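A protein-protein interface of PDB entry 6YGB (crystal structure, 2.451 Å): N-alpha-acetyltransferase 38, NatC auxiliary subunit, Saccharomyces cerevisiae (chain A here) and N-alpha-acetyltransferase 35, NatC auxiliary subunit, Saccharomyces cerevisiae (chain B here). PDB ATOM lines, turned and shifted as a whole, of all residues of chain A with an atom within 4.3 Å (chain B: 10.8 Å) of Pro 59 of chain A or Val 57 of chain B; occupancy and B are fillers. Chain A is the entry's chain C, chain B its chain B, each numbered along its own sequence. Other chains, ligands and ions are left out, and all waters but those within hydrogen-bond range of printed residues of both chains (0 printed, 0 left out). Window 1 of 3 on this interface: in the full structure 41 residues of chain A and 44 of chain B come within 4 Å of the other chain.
N of Asn 58 of chain B is in hydrogen-bond range of OD2 of Asp 63 of chain B (2.7 Å).
Of the printed residues of chain B, Leu 24 of chain A touches Val 57.
Of the printed residues of chain B, Val 56 of chain A touches Leu 55 and Val 57.
Of the printed residues of chain B, Ser 57 of chain A touches Leu 55, Glu 56 and Val 57.
Of the printed residues of chain B, Val 58 of chain A touches Val 57.
Of chain B, only Glu 56 (3.97 Å) and Val 57 (3.6 Å) come within 4 Å of Pro 59 of chain A.
Arg 60 of chain A touches none of the printed residues of chain B.
Of the printed residues of chain B, Arg 61 of chain A touches Asn 58.
Of chain B, only Val 57 and Asn 58 come within 4 Å of Ser 62 of chain A.
No residue of chain B comes within 4 Å of Val 63 of chain A.
Of the printed residues of chain A, Asn 58 of chain B touches Arg 61 and Ser 62.
Ser 65 of chain B touches none of the printed residues of chain A.
Among the printed residues, merely in contact across the chains: Pro 59 of chain A with Val 57 of chain B (3.6 Å), Val 56 of chain A with Leu 55 of chain B (3.6 Å), Val 56 of chain A with Val 57 of chain B (3.6 Å), Arg 61 of chain A with Asn 58 of chain B (3.6 Å), Leu 24 of chain A with Val 57 of chain B (3.7 Å), Ser 62 of chain A with Val 57 of chain B (3.8 Å), Val 58 of chain A with Val 57 of chain B (3.8 Å) and Pro 59 of chain A with Glu 56 of chain B (3.97 Å).
The backbone NH of Ser 57 of chain A lies within hydrogen-bond range of the backbone carbonyl oxygen of Leu 55 of chain B.
OE2 of Glu 56 of chain B lies close to OG of Ser 57 of chain A, at 3.5 Å.
The backbone carbonyl oxygen of Ser 57 of chain A is in hydrogen-bond range of the backbone NH of Val 57 of chain B, 3.3 Å away.
The side-chain amide nitrogen (ND2) of Asn 58 of chain B sits at hydrogen-bond distance from the side-chain hydroxyl (OG) of Ser 62 of chain A (3.0 Å).
Of the 11 printed residues of chain A, 7 touch a printed residue of chain B.
Hydrophobic or aromatic side chains of chain A within 4 Å of the printed part of chain B: Leu 24, Val 56, Val 58 and Pro 59.
Of the 22 printed residues of chain B, 4 touch a printed residue of chain A.
Hydrophobic or aromatic side chains of chain B within 4 Å of the printed part of chain A: Val 57.
Among the printed residues, 12 pairs touch across the chains.
Among the printed residues, no Asp or Glu carboxylate lies within 4 Å of a Lys or Arg side-chain nitrogen of the other chain.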
ATOM      1  N   LEU A  18      -1.933  15.758  23.113  1.00  0.00           N
ATOM      2  CA  LEU A  18      -2.748  15.067  22.129  1.00  0.00           C
ATOM      3  C   LEU A  18      -2.223  15.358  20.724  1.00  0.00           C
ATOM      4  O   LEU A  18      -1.245  16.086  20.538  1.00  0.00           O
ATOM      5  CB  LEU A  18      -4.217  15.462  22.280  1.00  0.00           C
ATOM      6  CG  LEU A  18      -4.839  15.208  23.661  1.00  0.00           C
ATOM      7  CD1 LEU A  18      -6.346  15.414  23.628  1.00  0.00           C
ATOM      8  CD2 LEU A  18      -4.496  13.814  24.175  1.00  0.00           C
ATOM      9  N   LEU A  24      -3.304  17.711  28.087  1.00  0.00           N
ATOM     10  CA  LEU A  24      -4.109  17.241  29.209  1.00  0.00           C
ATOM     11  C   LEU A  24      -3.195  16.929  30.385  1.00  0.00           C
ATOM     12  O   LEU A  24      -2.257  16.136  30.257  1.00  0.00           O
ATOM     13  CB  LEU A  24      -4.927  16.008  28.826  1.00  0.00           C
ATOM     14  CG  LEU A  24      -5.960  16.174  27.715  1.00  0.00           C
ATOM     15  CD1 LEU A  24      -6.663  14.856  27.469  1.00  0.00           C
ATOM     16  CD2 LEU A  24      -6.961  17.264  28.060  1.00  0.00           C
ATOM     17  N   ASN A  36      -4.477   2.385  26.517  1.00  0.00           N
ATOM     18  CA  ASN A  36      -5.568   3.327  26.732  1.00  0.00           C
ATOM     19  C   ASN A  36      -5.478   3.855  28.155  1.00  0.00           C
ATOM     20  O   ASN A  36      -5.331   3.077  29.102  1.00  0.00           O
ATOM     21  CB  ASN A  36      -6.925   2.658  26.507  1.00  0.00           C
ATOM     22  CG  ASN A  36      -7.067   2.067  25.119  1.00  0.00           C
ATOM     23  OD1 ASN A  36      -6.636   2.663  24.133  1.00  0.00           O
ATOM     24  ND2 ASN A  36      -7.674   0.885  25.037  1.00  0.00           N
ATOM     25  N   VAL A  56     -11.415  11.715  32.288  1.00  0.00           N
ATOM     26  CA  VAL A  56     -11.274  11.599  30.844  1.00  0.00           C
ATOM     27  C   VAL A  56     -10.510  10.328  30.519  1.00  0.00           C
ATOM     28  O   VAL A  56      -9.545   9.976  31.205  1.00  0.00           O
ATOM     29  CB  VAL A  56     -10.552  12.816  30.233  1.00  0.00           C
ATOM     30  CG1 VAL A  56     -10.759  12.838  28.727  1.00  0.00           C
ATOM     31  CG2 VAL A  56     -11.033  14.103  30.871  1.00  0.00           C
ATOM     32  N   SER A  57     -10.939   9.644  29.469  1.00  0.00           N
ATOM     33  CA  SER A  57     -10.234   8.494  28.938  1.00  0.00           C
ATOM     34  C   SER A  57      -9.563   8.912  27.639  1.00  0.00           C
ATOM     35  O   SER A  57     -10.176   9.584  26.805  1.00  0.00           O
ATOM     36  CB  SER A  57     -11.184   7.321  28.700  1.00  0.00           C
ATOM     37  OG  SER A  57     -12.115   7.622  27.678  1.00  0.00           O
ATOM     38  N   VAL A  58      -8.306   8.523  27.478  1.00  0.00           N
ATOM     39  CA  VAL A  58      -7.481   8.913  26.342  1.00  0.00           C
ATOM     40  C   VAL A  58      -7.083   7.651  25.587  1.00  0.00           C
ATOM     41  O   VAL A  58      -6.310   6.838  26.104  1.00  0.00           O
ATOM     42  CB  VAL A  58      -6.230   9.693  26.782  1.00  0.00           C
ATOM     43  CG1 VAL A  58      -5.567  10.334  25.589  1.00  0.00           C
ATOM     44  CG2 VAL A  58      -6.600  10.731  27.829  1.00  0.00           C
ATOM     45  N   PRO A  59      -7.573   7.443  24.364  1.00  0.00           N
ATOM     46  CA  PRO A  59      -7.190   6.251  23.597  1.00  0.00           C
ATOM     47  C   PRO A  59      -5.745   6.337  23.123  1.00  0.00           C
ATOM     48  O   PRO A  59      -5.116   7.396  23.131  1.00  0.00           O
ATOM     49  CB  PRO A  59      -8.163   6.257  22.412  1.00  0.00           C
ATOM     50  CG  PRO A  59      -9.268   7.180  22.818  1.00  0.00           C
ATOM     51  CD  PRO A  59      -8.648   8.203  23.711  1.00  0.00           C
ATOM     52  N   ARG A  60      -5.225   5.183  22.697  1.00  0.00           N
ATOM     53  CA  ARG A  60      -3.810   5.067  22.344  1.00  0.00           C
ATOM     54  C   ARG A  60      -3.439   5.980  21.179  1.00  0.00           C
ATOM     55  O   ARG A  60      -2.434   6.700  21.235  1.00  0.00           O
ATOM     56  CB  ARG A  60      -3.490   3.610  22.009  1.00  0.00           C
ATOM     57  CG  ARG A  60      -2.106   3.396  21.436  1.00  0.00           C
ATOM     58  CD  ARG A  60      -1.964   2.012  20.825  1.00  0.00           C
ATOM     59  NE  ARG A  60      -0.758   1.895  20.007  1.00  0.00           N
ATOM     60  CZ  ARG A  60       0.419   1.475  20.462  1.00  0.00           C
ATOM     61  NH1 ARG A  60       0.550   1.124  21.735  1.00  0.00           N
ATOM     62  NH2 ARG A  60       1.462   1.399  19.644  1.00  0.00           N
ATOM     63  N   ARG A  61      -4.232   5.946  20.104  1.00  0.00           N
ATOM     64  CA  ARG A  61      -3.947   6.761  18.926  1.00  0.00           C
ATOM     65  C   ARG A  61      -3.908   8.245  19.264  1.00  0.00           C
ATOM     66  O   ARG A  61      -3.120   8.998  18.680  1.00  0.00           O
ATOM     67  CB  ARG A  61      -5.001   6.508  17.846  1.00  0.00           C
ATOM     68  CG  ARG A  61      -4.791   7.319  16.577  1.00  0.00           C
ATOM     69  CD  ARG A  61      -6.103   7.692  15.895  1.00  0.00           C
ATOM     70  NE  ARG A  61      -6.760   8.834  16.530  1.00  0.00           N
ATOM     71  CZ  ARG A  61      -7.701   9.572  15.949  1.00  0.00           C
ATOM     72  NH1 ARG A  61      -8.094   9.295  14.713  1.00  0.00           N
ATOM     73  NH2 ARG A  61      -8.244  10.593  16.600  1.00  0.00           N
ATOM     74  N   SER A  62      -4.747   8.675  20.207  1.00  0.00           N
ATOM     75  CA  SER A  62      -4.897  10.078  20.564  1.00  0.00           C
ATOM     76  C   SER A  62      -3.735  10.621  21.383  1.00  0.00           C
ATOM     77  O   SER A  62      -3.624  11.843  21.527  1.00  0.00           O
ATOM     78  CB  SER A  62      -6.202  10.277  21.341  1.00  0.00           C
ATOM     79  OG  SER A  62      -7.316   9.844  20.583  1.00  0.00           O
ATOM     80  N   VAL A  63      -2.876   9.760  21.920  1.00  0.00           N
ATOM     81  CA  VAL A  63      -1.748  10.195  22.740  1.00  0.00           C
ATOM     82  C   VAL A  63      -0.578  10.544  21.826  1.00  0.00           C
ATOM     83  O   VAL A  63      -0.031   9.678  21.138  1.00  0.00           O
ATOM     84  CB  VAL A  63      -1.338   9.123  23.757  1.00  0.00           C
ATOM     85  CG1 VAL A  63      -0.024   9.509  24.417  1.00  0.00           C
ATOM     86  CG2 VAL A  63      -2.421   8.935  24.806  1.00  0.00           C
ATOM     87  N   THR B  25       6.914   8.409  27.015  1.00  0.00           N
ATOM     88  CA  THR B  25       6.097   7.721  26.019  1.00  0.00           C
ATOM     89  C   THR B  25       6.654   6.342  25.691  1.00  0.00           C
ATOM     90  O   THR B  25       5.937   5.337  25.739  1.00  0.00           O
ATOM     91  CB  THR B  25       6.000   8.570  24.752  1.00  0.00           C
ATOM     92  OG1 THR B  25       5.659   9.914  25.109  1.00  0.00           O
ATOM     93  CG2 THR B  25       4.931   8.016  23.822  1.00  0.00           C
ATOM     94  N   PHE B  28       6.275   3.797  28.555  1.00  0.00           N
ATOM     95  CA  PHE B  28       4.896   3.360  28.764  1.00  0.00           C
ATOM     96  C   PHE B  28       4.504   2.277  27.767  1.00  0.00           C
ATOM     97  O   PHE B  28       3.868   1.282  28.130  1.00  0.00           O
ATOM     98  CB  PHE B  28       3.951   4.557  28.653  1.00  0.00           C
ATOM     99  CG  PHE B  28       3.445   5.061  29.974  1.00  0.00           C
ATOM    100  CD1 PHE B  28       4.316   5.562  30.925  1.00  0.00           C
ATOM    101  CD2 PHE B  28       2.090   5.053  30.254  1.00  0.00           C
ATOM    102  CE1 PHE B  28       3.844   6.030  32.137  1.00  0.00           C
ATOM    103  CE2 PHE B  28       1.612   5.520  31.460  1.00  0.00           C
ATOM    104  CZ  PHE B  28       2.489   6.010  32.403  1.00  0.00           C
ATOM    105  N   CYS B  32       3.516  -1.497  28.655  1.00  0.00           N
ATOM    106  CA  CYS B  32       2.204  -1.963  28.216  1.00  0.00           C
ATOM    107  C   CYS B  32       2.307  -3.199  27.333  1.00  0.00           C
ATOM    108  O   CYS B  32       1.396  -4.035  27.332  1.00  0.00           O
ATOM    109  CB  CYS B  32       1.468  -0.842  27.481  1.00  0.00           C
ATOM    110  SG  CYS B  32       0.768   0.426  28.566  1.00  0.00           S
ATOM    111  N   SER B  54     -16.906   8.468  32.287  1.00  0.00           N
ATOM    112  CA  SER B  54     -15.753   9.196  31.785  1.00  0.00           C
ATOM    113  C   SER B  54     -15.991   9.719  30.372  1.00  0.00           C
ATOM    114  O   SER B  54     -16.758   9.150  29.590  1.00  0.00           O
ATOM    115  CB  SER B  54     -14.508   8.302  31.804  1.00  0.00           C
ATOM    116  OG  SER B  54     -14.714   7.137  31.029  1.00  0.00           O
ATOM    117  N   LEU B  55     -15.326  10.827  30.062  1.00  0.00           N
ATOM    118  CA  LEU B  55     -15.312  11.377  28.720  1.00  0.00           C
ATOM    119  C   LEU B  55     -14.242  10.674  27.894  1.00  0.00           C
ATOM    120  O   LEU B  55     -13.421   9.918  28.414  1.00  0.00           O
ATOM    121  CB  LEU B  55     -15.051  12.880  28.761  1.00  0.00           C
ATOM    122  CG  LEU B  55     -15.997  13.739  29.602  1.00  0.00           C
ATOM    123  CD1 LEU B  55     -15.386  15.109  29.821  1.00  0.00           C
ATOM    124  CD2 LEU B  55     -17.363  13.866  28.936  1.00  0.00           C
ATOM    125  N   GLU B  56     -14.246  10.939  26.590  1.00  0.00           N
ATOM    126  CA  GLU B  56     -13.255  10.354  25.698  1.00  0.00           C
ATOM    127  C   GLU B  56     -12.824  11.401  24.683  1.00  0.00           C
ATOM    128  O   GLU B  56     -13.667  11.989  24.001  1.00  0.00           O
ATOM    129  CB  GLU B  56     -13.805   9.112  24.993  1.00  0.00           C
ATOM    130  CG  GLU B  56     -12.726   8.174  24.492  1.00  0.00           C
ATOM    131  CD  GLU B  56     -13.276   6.825  24.099  1.00  0.00           C
ATOM    132  OE1 GLU B  56     -13.994   6.752  23.080  1.00  0.00           O
ATOM    133  OE2 GLU B  56     -13.002   5.840  24.814  1.00  0.00           O
ATOM    134  N   VAL B  57     -11.513  11.642  24.602  1.00  0.00           N
ATOM    135  CA  VAL B  57     -10.993  12.638  23.673  1.00  0.00           C
ATOM    136  C   VAL B  57     -11.119  12.121  22.247  1.00  0.00           C
ATOM    137  O   VAL B  57     -11.093  10.908  21.993  1.00  0.00           O
ATOM    138  CB  VAL B  57      -9.531  13.002  23.996  1.00  0.00           C
ATOM    139  CG1 VAL B  57      -9.410  13.521  25.417  1.00  0.00           C
ATOM    140  CG2 VAL B  57      -8.616  11.807  23.774  1.00  0.00           C
ATOM    141  N   ASN B  58     -11.271  13.055  21.307  1.00  0.00           N
ATOM    142  CA  ASN B  58     -11.359  12.746  19.877  1.00  0.00           C
ATOM    143  C   ASN B  58     -12.542  11.827  19.570  1.00  0.00           C
ATOM    144  O   ASN B  58     -12.475  10.958  18.701  1.00  0.00           O
ATOM    145  CB  ASN B  58     -10.042  12.162  19.360  1.00  0.00           C
ATOM    146  CG  ASN B  58      -8.897  13.159  19.446  1.00  0.00           C
ATOM    147  OD1 ASN B  58      -9.043  14.317  19.059  1.00  0.00           O
ATOM    148  ND2 ASN B  58      -7.758  12.719  19.968  1.00  0.00           N
ATOM    149  N   ASN B  59     -13.637  12.023  20.302  1.00  0.00           N
ATOM    150  CA  ASN B  59     -14.929  11.408  20.016  1.00  0.00           C
ATOM    151  C   ASN B  59     -15.952  12.529  19.971  1.00  0.00           C
ATOM    152  O   ASN B  59     -16.187  13.188  20.989  1.00  0.00           O
ATOM    153  CB  ASN B  59     -15.314  10.367  21.077  1.00  0.00           C
ATOM    154  CG  ASN B  59     -16.622   9.661  20.760  1.00  0.00           C
ATOM    155  OD1 ASN B  59     -17.614  10.294  20.393  1.00  0.00           O
ATOM    156  ND2 ASN B  59     -16.629   8.342  20.895  1.00  0.00           N
ATOM    157  N   SER B  60     -16.553  12.743  18.795  1.00  0.00           N
ATOM    158  CA  SER B  60     -17.432  13.893  18.590  1.00  0.00           C
ATOM    159  C   SER B  60     -18.518  13.973  19.656  1.00  0.00           C
ATOM    160  O   SER B  60     -18.790  15.051  20.199  1.00  0.00           O
ATOM    161  CB  SER B  60     -18.059  13.827  17.197  1.00  0.00           C
ATOM    162  OG  SER B  60     -17.110  13.406  16.233  1.00  0.00           O
ATOM    163  N   LYS B  61     -19.132  12.841  19.984  1.00  0.00           N
ATOM    164  CA  LYS B  61     -20.259  12.815  20.903  1.00  0.00           C
ATOM    165  C   LYS B  61     -19.837  12.793  22.368  1.00  0.00           C
ATOM    166  O   LYS B  61     -20.691  12.965  23.244  1.00  0.00           O
ATOM    167  CB  LYS B  61     -21.148  11.613  20.569  1.00  0.00           C
ATOM    168  CG  LYS B  61     -21.563  11.578  19.093  1.00  0.00           C
ATOM    169  CD  LYS B  61     -21.940  10.177  18.618  1.00  0.00           C
ATOM    170  CE  LYS B  61     -23.401   9.855  18.891  1.00  0.00           C
ATOM    171  NZ  LYS B  61     -23.749   8.470  18.462  1.00  0.00           N
ATOM    172  N   LEU B  62     -18.548  12.620  22.656  1.00  0.00           N
ATOM    173  CA  LEU B  62     -18.059  12.606  24.026  1.00  0.00           C
ATOM    174  C   LEU B  62     -16.970  13.636  24.304  1.00  0.00           C
ATOM    175  O   LEU B  62     -16.531  13.748  25.455  1.00  0.00           O
ATOM    176  CB  LEU B  62     -17.534  11.212  24.394  1.00  0.00           C
ATOM    177  CG  LEU B  62     -18.594  10.136  24.630  1.00  0.00           C
ATOM    178  CD1 LEU B  62     -17.964   8.753  24.706  1.00  0.00           C
ATOM    179  CD2 LEU B  62     -19.382  10.429  25.898  1.00  0.00           C
ATOM    180  N   ASP B  63     -16.520  14.390  23.302  1.00  0.00           N
ATOM    181  CA  ASP B  63     -15.463  15.384  23.469  1.00  0.00           C
ATOM    182  C   ASP B  63     -16.050  16.780  23.283  1.00  0.00           C
ATOM    183  O   ASP B  63     -16.540  17.110  22.200  1.00  0.00           O
ATOM    184  CB  ASP B  63     -14.326  15.141  22.473  1.00  0.00           C
ATOM    185  CG  ASP B  63     -13.039  15.878  22.846  1.00  0.00           C
ATOM    186  OD1 ASP B  63     -13.112  16.919  23.529  1.00  0.00           O
ATOM    187  OD2 ASP B  63     -11.953  15.419  22.442  1.00  0.00           O
ATOM    188  N   SER B  64     -15.975  17.607  24.331  1.00  0.00           N
ATOM    189  CA  SER B  64     -16.525  18.961  24.282  1.00  0.00           C
ATOM    190  C   SER B  64     -15.682  19.890  23.411  1.00  0.00           C
ATOM    191  O   SER B  64     -16.202  20.874  22.866  1.00  0.00           O
ATOM    192  CB  SER B  64     -16.644  19.521  25.706  1.00  0.00           C
ATOM    193  OG  SER B  64     -17.276  18.584  26.570  1.00  0.00           O
ATOM    194  N   SER B  65     -14.398  19.595  23.267  1.00  0.00           N
ATOM    195  CA  SER B  65     -13.474  20.430  22.522  1.00  0.00           C
ATOM    196  C   SER B  65     -13.681  20.361  21.015  1.00  0.00           C
ATOM    197  O   SER B  65     -13.200  21.248  20.301  1.00  0.00           O
ATOM    198  CB  SER B  65     -12.040  20.025  22.866  1.00  0.00           C
ATOM    199  OG  SER B  65     -11.832  20.006  24.272  1.00  0.00           O
ATOM    200  N   LEU B  66     -14.373  19.342  20.513  1.00  0.00           N
ATOM    201  CA  LEU B  66     -14.582  19.187  19.079  1.00  0.00           C
ATOM    202  C   LEU B  66     -15.859  19.850  18.585  1.00  0.00           C
ATOM    203  O   LEU B  66     -16.202  19.685  17.409  1.00  0.00           O
ATOM    204  CB  LEU B  66     -14.604  17.701  18.702  1.00  0.00           C
ATOM    205  CG  LEU B  66     -13.409  16.875  19.172  1.00  0.00           C
ATOM    206  CD1 LEU B  66     -13.472  15.470  18.592  1.00  0.00           C
ATOM    207  CD2 LEU B  66     -12.099  17.561  18.812  1.00  0.00           C
ATOM    208  N   ILE B  67     -16.571  20.578  19.452  1.00  0.00           N
ATOM    209  CA  ILE B  67     -17.801  21.246  19.045  1.00  0.00           C
ATOM    210  C   ILE B  67     -17.522  22.201  17.897  1.00  0.00           C
ATOM    211  O   ILE B  67     -16.616  23.041  17.974  1.00  0.00           O
ATOM    212  CB  ILE B  67     -18.413  21.989  20.240  1.00  0.00           C
ATOM    213  CG1 ILE B  67     -18.998  21.001  21.249  1.00  0.00           C
ATOM    214  CG2 ILE B  67     -19.466  22.983  19.774  1.00  0.00           C
ATOM    215  CD1 ILE B  67     -19.506  21.663  22.505  1.00  0.00           C
ATOM    216  N   ASN B 283     -15.904  21.856  31.821  1.00  0.00           N
ATOM    217  CA  ASN B 283     -17.082  21.035  31.575  1.00  0.00           C
ATOM    218  C   ASN B 283     -16.685  19.574  31.709  1.00  0.00           C
ATOM    219  O   ASN B 283     -15.834  19.092  30.955  1.00  0.00           O
ATOM    220  CB  ASN B 283     -17.662  21.325  30.188  1.00  0.00           C
ATOM    221  CG  ASN B 283     -18.893  20.500  29.878  1.00  0.00           C
ATOM    222  OD1 ASN B 283     -19.484  19.880  30.764  1.00  0.00           O
ATOM    223  ND2 ASN B 283     -19.291  20.494  28.611  1.00  0.00           N
ATOM    224  N   GLN B 284     -17.290  18.877  32.671  1.00  0.00           N
ATOM    225  CA  GLN B 284     -17.036  17.458  32.880  1.00  0.00           C
ATOM    226  C   GLN B 284     -18.036  16.574  32.152  1.00  0.00           C
ATOM    227  O   GLN B 284     -18.006  15.353  32.328  1.00  0.00           O
ATOM    228  CB  GLN B 284     -17.063  17.118  34.375  1.00  0.00           C
ATOM    229  CG  GLN B 284     -15.990  17.799  35.210  1.00  0.00           C
ATOM    230  CD  GLN B 284     -15.859  17.195  36.605  1.00  0.00           C
ATOM    231  OE1 GLN B 284     -16.090  15.999  36.803  1.00  0.00           O
ATOM    232  NE2 GLN B 284     -15.484  18.022  37.575  1.00  0.00           N
ATOM    233  N   PHE B 285     -18.909  17.154  31.344  1.00  0.00           N
ATOM    234  CA  PHE B 285     -19.988  16.434  30.699  1.00  0.00           C
ATOM    235  C   PHE B 285     -19.820  16.430  29.182  1.00  0.00           C
ATOM    236  O   PHE B 285     -19.066  17.236  28.626  1.00  0.00           O
ATOM    237  CB  PHE B 285     -21.335  17.066  31.076  1.00  0.00           C
ATOM    238  CG  PHE B 285     -21.694  16.911  32.529  1.00  0.00           C
ATOM    239  CD1 PHE B 285     -21.192  17.786  33.477  1.00  0.00           C
ATOM    240  CD2 PHE B 285     -22.532  15.888  32.947  1.00  0.00           C
ATOM    241  CE1 PHE B 285     -21.522  17.647  34.815  1.00  0.00           C
ATOM    242  CE2 PHE B 285     -22.864  15.745  34.283  1.00  0.00           C
ATOM    243  CZ  PHE B 285     -22.359  16.626  35.218  1.00  0.00           C
ATOM    244  N   PRO B 286     -20.491  15.515  28.483  1.00  0.00           N
ATOM    245  CA  PRO B 286     -20.391  15.474  27.018  1.00  0.00           C
ATOM    246  C   PRO B 286     -21.073  16.676  26.394  1.00  0.00           C
ATOM    247  O   PRO B 286     -21.923  17.315  27.033  1.00  0.00           O
ATOM    248  CB  PRO B 286     -21.117  14.169  26.650  1.00  0.00           C
ATOM    249  CG  PRO B 286     -21.145  13.365  27.908  1.00  0.00           C
ATOM    250  CD  PRO B 286     -21.238  14.361  29.016  1.00  0.00           C
ATOM    251  N   PRO B 287     -20.721  17.030  25.157  1.00  0.00           N
ATOM    252  CA  PRO B 287     -21.429  18.122  24.484  1.00  0.00           C
ATOM    253  C   PRO B 287     -22.885  17.753  24.271  1.00  0.00           C
ATOM    254  O   PRO B 287     -23.216  16.599  23.995  1.00  0.00           O
ATOM    255  CB  PRO B 287     -20.687  18.263  23.151  1.00  0.00           C
ATOM    256  CG  PRO B 287     -20.058  16.930  22.930  1.00  0.00           C
ATOM    257  CD  PRO B 287     -19.684  16.434  24.295  1.00  0.00           C
